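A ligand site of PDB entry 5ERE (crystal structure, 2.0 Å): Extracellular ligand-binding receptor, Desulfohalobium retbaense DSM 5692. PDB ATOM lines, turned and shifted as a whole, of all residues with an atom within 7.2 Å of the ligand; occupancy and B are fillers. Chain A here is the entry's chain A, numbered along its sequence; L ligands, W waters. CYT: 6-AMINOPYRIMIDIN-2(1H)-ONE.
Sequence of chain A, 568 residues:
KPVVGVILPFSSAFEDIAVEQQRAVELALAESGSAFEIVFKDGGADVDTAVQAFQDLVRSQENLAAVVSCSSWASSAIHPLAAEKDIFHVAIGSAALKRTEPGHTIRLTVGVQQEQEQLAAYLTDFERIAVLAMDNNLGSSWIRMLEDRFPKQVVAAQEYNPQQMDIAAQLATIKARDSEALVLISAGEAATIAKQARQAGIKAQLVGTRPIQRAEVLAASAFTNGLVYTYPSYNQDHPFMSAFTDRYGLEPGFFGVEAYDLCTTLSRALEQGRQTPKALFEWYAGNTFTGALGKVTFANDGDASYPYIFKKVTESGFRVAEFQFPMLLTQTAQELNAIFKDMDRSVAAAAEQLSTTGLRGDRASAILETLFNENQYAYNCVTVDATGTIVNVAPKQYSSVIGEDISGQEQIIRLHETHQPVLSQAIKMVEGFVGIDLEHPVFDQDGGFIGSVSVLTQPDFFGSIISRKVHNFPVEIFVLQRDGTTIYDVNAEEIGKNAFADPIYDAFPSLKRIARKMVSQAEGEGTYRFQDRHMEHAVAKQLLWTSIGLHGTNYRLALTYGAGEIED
OE1 of Glu 431 sits at hydrogen-bond distance from N3 of the ligand, at 2.7 Å. A nitrogen (N1) of the ligand sits close to the side-chain amide oxygen (OE1) of Gln 409 (2.7 Å). The backbone NH (N) of Val 430 is in hydrogen-bond range of an oxygen (O2) of the ligand (3.0 Å). The side-chain amide oxygen (OD1) of Asn 380 is in hydrogen-bond range of a nitrogen (N4) of the ligand, at 3.3 Å. SD of Met 429 sits close to N1 of the ligand (3.5 Å).
The side-chain carboxylate of Glu 431 sits at hydrogen-bond distance from the side-chain amide nitrogen of Asn 380, at 3.1 Å. The side-chain amide nitrogen (NE2) of Gln 411 lies within hydrogen-bond range of the side-chain amide oxygen (OE1) of Gln 409 (2.9 Å). OD2 of Asp 437 sits close to OE2 of Glu 439, at 2.5 Å. OD2 of Asp 437 is in hydrogen-bond range of NE2 of Gln 411. The backbone carbonyl oxygen (O) of Asn 380 lies within hydrogen-bond range of the backbone NH (N) of Leu 456. The backbone NH (N) of Ser 454 lies within hydrogen-bond range of the backbone carbonyl oxygen (O) of Val 382 (2.9 Å). The backbone carbonyl oxygen of Leu 456 sits at hydrogen-bond distance from the backbone NH of Tyr 379 (2.7 Å).
Residues that only touch the ligand: Val 382, Ile 406, Asp 437, Glu 439, Ser 454 and Leu 456. Hydrophobic or aromatic side chains that line the ligand: Val 382, Ile 406, Met 429, Val 430 and Leu 456. Of the 26 residues printed, 11 come within 4 Å of the ligand.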
ATOM      1  N   TYR A 379      -6.938  -9.156   2.731  1.00  0.00           N
ATOM      2  CA  TYR A 379      -6.189  -9.223   1.511  1.00  0.00           C
ATOM      3  C   TYR A 379      -5.847  -7.794   1.093  1.00  0.00           C
ATOM      4  O   TYR A 379      -4.722  -7.524   0.711  1.00  0.00           O
ATOM      5  CB  TYR A 379      -7.032  -9.913   0.448  1.00  0.00           C
ATOM      6  CG  TYR A 379      -6.330 -10.039  -0.868  1.00  0.00           C
ATOM      7  CD1 TYR A 379      -5.443 -11.071  -1.098  1.00  0.00           C
ATOM      8  CD2 TYR A 379      -6.554  -9.121  -1.872  1.00  0.00           C
ATOM      9  CE1 TYR A 379      -4.814 -11.216  -2.304  1.00  0.00           C
ATOM     10  CE2 TYR A 379      -5.909  -9.246  -3.106  1.00  0.00           C
ATOM     11  CZ  TYR A 379      -5.057 -10.310  -3.309  1.00  0.00           C
ATOM     12  OH  TYR A 379      -4.416 -10.442  -4.506  1.00  0.00           O
ATOM     13  N   ASN A 380      -6.836  -6.895   1.138  1.00  0.00           N
ATOM     14  CA  ASN A 380      -6.530  -5.472   1.053  1.00  0.00           C
ATOM     15  C   ASN A 380      -7.666  -4.599   1.575  1.00  0.00           C
ATOM     16  O   ASN A 380      -8.705  -5.099   2.013  1.00  0.00           O
ATOM     17  CB  ASN A 380      -6.158  -5.055  -0.383  1.00  0.00           C
ATOM     18  CG  ASN A 380      -7.301  -5.183  -1.388  1.00  0.00           C
ATOM     19  OD1 ASN A 380      -8.468  -5.142  -1.060  1.00  0.00           O
ATOM     20  ND2 ASN A 380      -6.932  -5.284  -2.654  1.00  0.00           N
ATOM     21  N   CYS A 381      -7.441  -3.295   1.528  1.00  0.00           N
ATOM     22  CA  CYS A 381      -8.394  -2.295   1.966  1.00  0.00           C
ATOM     23  C   CYS A 381      -8.536  -1.209   0.920  1.00  0.00           C
ATOM     24  O   CYS A 381      -7.539  -0.756   0.337  1.00  0.00           O
ATOM     25  CB  CYS A 381      -7.956  -1.668   3.314  1.00  0.00           C
ATOM     26  SG  CYS A 381      -7.656  -2.819   4.664  1.00  0.00           S
ATOM     27  N   VAL A 382      -9.771  -0.803   0.675  1.00  0.00           N
ATOM     28  CA  VAL A 382     -10.037   0.227  -0.297  1.00  0.00           C
ATOM     29  C   VAL A 382     -11.000   1.271   0.205  1.00  0.00           C
ATOM     30  O   VAL A 382     -11.765   1.052   1.184  1.00  0.00           O
ATOM     31  CB  VAL A 382     -10.597  -0.335  -1.609  1.00  0.00           C
ATOM     32  CG1 VAL A 382      -9.650  -1.336  -2.220  1.00  0.00           C
ATOM     33  CG2 VAL A 382     -11.970  -0.976  -1.376  1.00  0.00           C
ATOM     34  N   VAL A 384     -14.036   3.684  -1.665  1.00  0.00           N
ATOM     35  CA  VAL A 384     -14.966   3.616  -2.787  1.00  0.00           C
ATOM     36  C   VAL A 384     -15.855   4.859  -2.751  1.00  0.00           C
ATOM     37  O   VAL A 384     -16.510   5.112  -1.733  1.00  0.00           O
ATOM     38  CB  VAL A 384     -15.859   2.347  -2.705  1.00  0.00           C
ATOM     39  CG1 VAL A 384     -16.797   2.257  -3.922  1.00  0.00           C
ATOM     40  CG2 VAL A 384     -15.010   1.095  -2.605  1.00  0.00           C
ATOM     41  N   ILE A 390     -13.706   2.372  -6.969  1.00  0.00           N
ATOM     42  CA  ILE A 390     -12.567   2.285  -6.075  1.00  0.00           C
ATOM     43  C   ILE A 390     -11.597   3.421  -6.391  1.00  0.00           C
ATOM     44  O   ILE A 390     -11.167   3.563  -7.530  1.00  0.00           O
ATOM     45  CB  ILE A 390     -11.836   0.930  -6.202  1.00  0.00           C
ATOM     46  CG1 ILE A 390     -12.799  -0.206  -5.828  1.00  0.00           C
ATOM     47  CG2 ILE A 390     -10.626   0.920  -5.296  1.00  0.00           C
ATOM     48  CD1 ILE A 390     -12.209  -1.594  -5.977  1.00  0.00           C
ATOM     49  N   VAL A 393      -6.428   2.343  -2.350  1.00  0.00           N
ATOM     50  CA  VAL A 393      -6.178   0.981  -1.871  1.00  0.00           C
ATOM     51  C   VAL A 393      -4.867   0.887  -1.120  1.00  0.00           C
ATOM     52  O   VAL A 393      -3.898   1.538  -1.476  1.00  0.00           O
ATOM     53  CB  VAL A 393      -6.154  -0.032  -3.036  1.00  0.00           C
ATOM     54  CG1 VAL A 393      -5.015   0.286  -4.032  1.00  0.00           C
ATOM     55  CG2 VAL A 393      -6.011  -1.481  -2.507  1.00  0.00           C
ATOM     56  N   VAL A 401      -6.409  -1.911  -9.066  1.00  0.00           N
ATOM     57  CA  VAL A 401      -7.858  -1.959  -8.842  1.00  0.00           C
ATOM     58  C   VAL A 401      -8.420  -0.532  -8.766  1.00  0.00           C
ATOM     59  O   VAL A 401      -9.615  -0.351  -8.876  1.00  0.00           O
ATOM     60  CB  VAL A 401      -8.224  -2.770  -7.565  1.00  0.00           C
ATOM     61  CG1 VAL A 401      -7.549  -4.117  -7.623  1.00  0.00           C
ATOM     62  CG2 VAL A 401      -7.814  -2.019  -6.291  1.00  0.00           C
ATOM     63  N   GLU A 404     -11.624   0.831 -10.724  1.00  0.00           N
ATOM     64  CA  GLU A 404     -12.596  -0.219 -10.987  1.00  0.00           C
ATOM     65  C   GLU A 404     -14.010   0.151 -10.495  1.00  0.00           C
ATOM     66  O   GLU A 404     -14.200   0.607  -9.367  1.00  0.00           O
ATOM     67  CB  GLU A 404     -12.123  -1.528 -10.360  1.00  0.00           C
ATOM     68  CG  GLU A 404     -11.000  -2.216 -11.132  1.00  0.00           C
ATOM     69  CD  GLU A 404     -11.500  -3.104 -12.258  1.00  0.00           C
ATOM     70  OE1 GLU A 404     -12.738  -3.161 -12.482  1.00  0.00           O
ATOM     71  OE2 GLU A 404     -10.671  -3.750 -12.925  1.00  0.00           O
ATOM     72  N   ILE A 406     -17.316  -0.983  -9.128  1.00  0.00           N
ATOM     73  CA  ILE A 406     -17.935  -2.098  -8.387  1.00  0.00           C
ATOM     74  C   ILE A 406     -19.345  -1.721  -7.931  1.00  0.00           C
ATOM     75  O   ILE A 406     -19.869  -2.260  -6.942  1.00  0.00           O
ATOM     76  CB  ILE A 406     -17.044  -2.516  -7.180  1.00  0.00           C
ATOM     77  CG1 ILE A 406     -16.950  -1.382  -6.152  1.00  0.00           C
ATOM     78  CG2 ILE A 406     -15.615  -2.902  -7.671  1.00  0.00           C
ATOM     79  CD1 ILE A 406     -16.277  -1.766  -4.866  1.00  0.00           C
ATOM     80  N   GLN A 409     -21.865  -4.582  -7.500  1.00  0.00           N
ATOM     81  CA  GLN A 409     -21.685  -5.645  -6.517  1.00  0.00           C
ATOM     82  C   GLN A 409     -22.829  -5.570  -5.475  1.00  0.00           C
ATOM     83  O   GLN A 409     -23.220  -4.494  -5.016  1.00  0.00           O
ATOM     84  CB  GLN A 409     -20.300  -5.550  -5.854  1.00  0.00           C
ATOM     85  CG  GLN A 409     -19.160  -5.874  -6.845  1.00  0.00           C
ATOM     86  CD  GLN A 409     -17.764  -5.958  -6.207  1.00  0.00           C
ATOM     87  OE1 GLN A 409     -17.587  -5.794  -4.995  1.00  0.00           O
ATOM     88  NE2 GLN A 409     -16.769  -6.184  -7.043  1.00  0.00           N
ATOM     89  N   GLN A 411     -23.365  -6.089  -2.314  1.00  0.00           N
ATOM     90  CA  GLN A 411     -23.164  -5.386  -1.037  1.00  0.00           C
ATOM     91  C   GLN A 411     -23.041  -3.879  -1.214  1.00  0.00           C
ATOM     92  O   GLN A 411     -23.405  -3.107  -0.325  1.00  0.00           O
ATOM     93  CB  GLN A 411     -21.933  -5.913  -0.291  1.00  0.00           C
ATOM     94  CG  GLN A 411     -20.550  -5.346  -0.702  1.00  0.00           C
ATOM     95  CD  GLN A 411     -20.051  -5.926  -2.019  1.00  0.00           C
ATOM     96  OE1 GLN A 411     -20.814  -6.557  -2.738  1.00  0.00           O
ATOM     97  NE2 GLN A 411     -18.756  -5.774  -2.289  1.00  0.00           N
ATOM     98  N   ILE A 412     -22.525  -3.462  -2.378  1.00  0.00           N
ATOM     99  CA  ILE A 412     -22.282  -2.055  -2.667  1.00  0.00           C
ATOM    100  C   ILE A 412     -23.622  -1.368  -2.949  1.00  0.00           C
ATOM    101  O   ILE A 412     -23.862  -0.231  -2.542  1.00  0.00           O
ATOM    102  CB  ILE A 412     -21.324  -1.876  -3.886  1.00  0.00           C
ATOM    103  CG1 ILE A 412     -19.912  -2.379  -3.590  1.00  0.00           C
ATOM    104  CG2 ILE A 412     -21.300  -0.418  -4.372  1.00  0.00           C
ATOM    105  CD1 ILE A 412     -19.184  -1.626  -2.524  1.00  0.00           C
ATOM    106  N   ILE A 427     -18.482 -13.422  -3.239  1.00  0.00           N
ATOM    107  CA  ILE A 427     -18.680 -13.088  -4.651  1.00  0.00           C
ATOM    108  C   ILE A 427     -17.302 -12.879  -5.260  1.00  0.00           C
ATOM    109  O   ILE A 427     -16.320 -12.722  -4.545  1.00  0.00           O
ATOM    110  CB  ILE A 427     -19.554 -11.806  -4.851  1.00  0.00           C
ATOM    111  CG1 ILE A 427     -18.909 -10.584  -4.148  1.00  0.00           C
ATOM    112  CG2 ILE A 427     -21.007 -12.021  -4.354  1.00  0.00           C
ATOM    113  CD1 ILE A 427     -19.587  -9.234  -4.454  1.00  0.00           C
ATOM    114  N   LYS A 428     -17.242 -12.873  -6.582  1.00  0.00           N
ATOM    115  CA  LYS A 428     -15.975 -12.638  -7.297  1.00  0.00           C
ATOM    116  C   LYS A 428     -15.556 -11.170  -7.179  1.00  0.00           C
ATOM    117  O   LYS A 428     -16.307 -10.252  -7.499  1.00  0.00           O
ATOM    118  CB  LYS A 428     -16.107 -13.075  -8.767  1.00  0.00           C
ATOM    119  CG  LYS A 428     -14.809 -12.945  -9.601  1.00  0.00           C
ATOM    120  CD  LYS A 428     -13.780 -14.030  -9.296  1.00  0.00           C
ATOM    121  CE  LYS A 428     -12.549 -13.914 -10.196  1.00  0.00           C
ATOM    122  NZ  LYS A 428     -12.795 -14.301 -11.621  1.00  0.00           N
ATOM    123  N   MET A 429     -14.355 -10.955  -6.679  1.00  0.00           N
ATOM    124  CA  MET A 429     -13.840  -9.618  -6.482  1.00  0.00           C
ATOM    125  C   MET A 429     -12.929  -9.226  -7.671  1.00  0.00           C
ATOM    126  O   MET A 429     -12.402 -10.107  -8.338  1.00  0.00           O
ATOM    127  CB  MET A 429     -13.068  -9.579  -5.161  1.00  0.00           C
ATOM    128  CG  MET A 429     -13.895  -9.987  -3.953  1.00  0.00           C
ATOM    129  SD  MET A 429     -15.259  -8.634  -3.538  1.00  0.00           S
ATOM    130  CE  MET A 429     -16.224  -9.600  -2.112  1.00  0.00           C
ATOM    131  N   VAL A 430     -12.725  -7.921  -7.916  1.00  0.00           N
ATOM    132  CA  VAL A 430     -11.838  -7.476  -9.014  1.00  0.00           C
ATOM    133  C   VAL A 430     -10.423  -7.981  -8.833  1.00  0.00           C
ATOM    134  O   VAL A 430      -9.662  -8.089  -9.806  1.00  0.00           O
ATOM    135  CB  VAL A 430     -11.781  -5.932  -9.172  1.00  0.00           C
ATOM    136  CG1 VAL A 430     -13.100  -5.385  -9.642  1.00  0.00           C
ATOM    137  CG2 VAL A 430     -11.326  -5.244  -7.894  1.00  0.00           C
ATOM    138  N   GLU A 431     -10.077  -8.291  -7.575  1.00  0.00           N
ATOM    139  CA  GLU A 431      -8.758  -8.812  -7.236  1.00  0.00           C
ATOM    140  C   GLU A 431      -8.485 -10.210  -7.783  1.00  0.00           C
ATOM    141  O   GLU A 431      -7.338 -10.658  -7.761  1.00  0.00           O
ATOM    142  CB  GLU A 431      -8.573  -8.801  -5.718  1.00  0.00           C
ATOM    143  CG  GLU A 431      -8.390  -7.421  -5.135  1.00  0.00           C
ATOM    144  CD  GLU A 431      -9.647  -6.616  -4.910  1.00  0.00           C
ATOM    145  OE1 GLU A 431     -10.801  -7.082  -5.177  1.00  0.00           O
ATOM    146  OE2 GLU A 431      -9.473  -5.477  -4.438  1.00  0.00           O
ATOM    147  N   GLY A 432      -9.539 -10.897  -8.256  1.00  0.00           N
ATOM    148  CA  GLY A 432      -9.407 -12.181  -8.929  1.00  0.00           C
ATOM    149  C   GLY A 432      -9.800 -13.443  -8.182  1.00  0.00           C
ATOM    150  O   GLY A 432      -9.387 -14.535  -8.557  1.00  0.00           O
ATOM    151  N   PHE A 433     -10.584 -13.317  -7.113  1.00  0.00           N
ATOM    152  CA  PHE A 433     -11.013 -14.504  -6.378  1.00  0.00           C
ATOM    153  C   PHE A 433     -12.380 -14.279  -5.715  1.00  0.00           C
ATOM    154  O   PHE A 433     -12.850 -13.141  -5.599  1.00  0.00           O
ATOM    155  CB  PHE A 433      -9.938 -14.903  -5.346  1.00  0.00           C
ATOM    156  CG  PHE A 433      -9.707 -13.884  -4.233  1.00  0.00           C
ATOM    157  CD1 PHE A 433     -10.519 -13.897  -3.082  1.00  0.00           C
ATOM    158  CD2 PHE A 433      -8.729 -12.911  -4.345  1.00  0.00           C
ATOM    159  CE1 PHE A 433     -10.322 -12.975  -2.051  1.00  0.00           C
ATOM    160  CE2 PHE A 433      -8.531 -11.975  -3.314  1.00  0.00           C
ATOM    161  CZ  PHE A 433      -9.332 -12.003  -2.178  1.00  0.00           C
ATOM    162  N   ASP A 437     -16.317  -9.112   1.536  1.00  0.00           N
ATOM    163  CA  ASP A 437     -16.066  -7.687   1.729  1.00  0.00           C
ATOM    164  C   ASP A 437     -16.871  -7.122   2.915  1.00  0.00           C
ATOM    165  O   ASP A 437     -18.086  -7.314   2.970  1.00  0.00           O
ATOM    166  CB  ASP A 437     -16.451  -6.938   0.431  1.00  0.00           C
ATOM    167  CG  ASP A 437     -16.151  -5.420   0.487  1.00  0.00           C
ATOM    168  OD1 ASP A 437     -15.278  -5.008   1.255  1.00  0.00           O
ATOM    169  OD2 ASP A 437     -16.784  -4.664  -0.263  1.00  0.00           O
ATOM    170  N   LEU A 438     -16.208  -6.456   3.860  1.00  0.00           N
ATOM    171  CA  LEU A 438     -16.900  -5.735   4.928  1.00  0.00           C
ATOM    172  C   LEU A 438     -16.734  -4.255   4.684  1.00  0.00           C
ATOM    173  O   LEU A 438     -15.594  -3.763   4.614  1.00  0.00           O
ATOM    174  CB  LEU A 438     -16.352  -6.139   6.308  1.00  0.00           C
ATOM    175  CG  LEU A 438     -16.841  -5.377   7.548  1.00  0.00           C
ATOM    176  CD1 LEU A 438     -18.319  -5.373   7.692  1.00  0.00           C
ATOM    177  CD2 LEU A 438     -16.209  -6.013   8.763  1.00  0.00           C
ATOM    178  N   GLU A 439     -17.846  -3.536   4.532  1.00  0.00           N
ATOM    179  CA  GLU A 439     -17.803  -2.092   4.244  1.00  0.00           C
ATOM    180  C   GLU A 439     -18.578  -1.235   5.230  1.00  0.00           C
ATOM    181  O   GLU A 439     -19.672  -1.607   5.673  1.00  0.00           O
ATOM    182  CB  GLU A 439     -18.327  -1.784   2.855  1.00  0.00           C
ATOM    183  CG  GLU A 439     -17.627  -2.527   1.719  1.00  0.00           C
ATOM    184  CD  GLU A 439     -17.155  -1.635   0.559  1.00  0.00           C
ATOM    185  OE1 GLU A 439     -17.186  -0.384   0.659  1.00  0.00           O
ATOM    186  OE2 GLU A 439     -16.699  -2.199  -0.470  1.00  0.00           O
ATOM    187  N   SER A 454     -13.578  -0.266   2.968  1.00  0.00           N
ATOM    188  CA  SER A 454     -13.672  -1.738   2.868  1.00  0.00           C
ATOM    189  C   SER A 454     -12.474  -2.534   3.397  1.00  0.00           C
ATOM    190  O   SER A 454     -11.320  -2.101   3.279  1.00  0.00           O
ATOM    191  CB  SER A 454     -13.871  -2.095   1.401  1.00  0.00           C
ATOM    192  OG  SER A 454     -13.506  -3.444   1.105  1.00  0.00           O
ATOM    193  N   VAL A 455     -12.751  -3.683   4.018  1.00  0.00           N
ATOM    194  CA  VAL A 455     -11.744  -4.746   4.187  1.00  0.00           C
ATOM    195  C   VAL A 455     -12.250  -5.928   3.386  1.00  0.00           C
ATOM    196  O   VAL A 455     -13.350  -6.380   3.613  1.00  0.00           O
ATOM    197  CB  VAL A 455     -11.540  -5.201   5.655  1.00  0.00           C
ATOM    198  CG1 VAL A 455     -10.628  -6.424   5.738  1.00  0.00           C
ATOM    199  CG2 VAL A 455     -10.896  -4.070   6.471  1.00  0.00           C
ATOM    200  N   LEU A 456     -11.418  -6.371   2.441  1.00  0.00           N
ATOM    201  CA  LEU A 456     -11.642  -7.592   1.705  1.00  0.00           C
ATOM    202  C   LEU A 456     -10.822  -8.720   2.349  1.00  0.00           C
ATOM    203  O   LEU A 456      -9.611  -8.603   2.544  1.00  0.00           O
ATOM    204  CB  LEU A 456     -11.263  -7.398   0.221  1.00  0.00           C
ATOM    205  CG  LEU A 456     -11.110  -8.651  -0.620  1.00  0.00           C
ATOM    206  CD1 LEU A 456     -12.416  -9.389  -0.748  1.00  0.00           C
ATOM    207  CD2 LEU A 456     -10.554  -8.291  -2.029  1.00  0.00           C
HETATM  208  N3  CYT L   1     -12.740  -5.497  -4.167  1.00  0.00           N
HETATM  209  C4  CYT L   1     -12.603  -4.823  -3.029  1.00  0.00           C
HETATM  210  N1  CYT L   1     -15.102  -5.191  -4.050  1.00  0.00           N
HETATM  211  C2  CYT L   1     -13.978  -5.707  -4.711  1.00  0.00           C
HETATM  212  O2  CYT L   1     -14.131  -6.364  -5.760  1.00  0.00           O
HETATM  213  N4  CYT L   1     -11.345  -4.637  -2.545  1.00  0.00           N
HETATM  214  C5  CYT L   1     -13.749  -4.289  -2.337  1.00  0.00           C
HETATM  215  C6  CYT L   1     -14.964  -4.495  -2.875  1.00  0.00           C
HETATM  216  O   HOH W   1     -10.942  -3.884   0.144  1.00  0.00           O
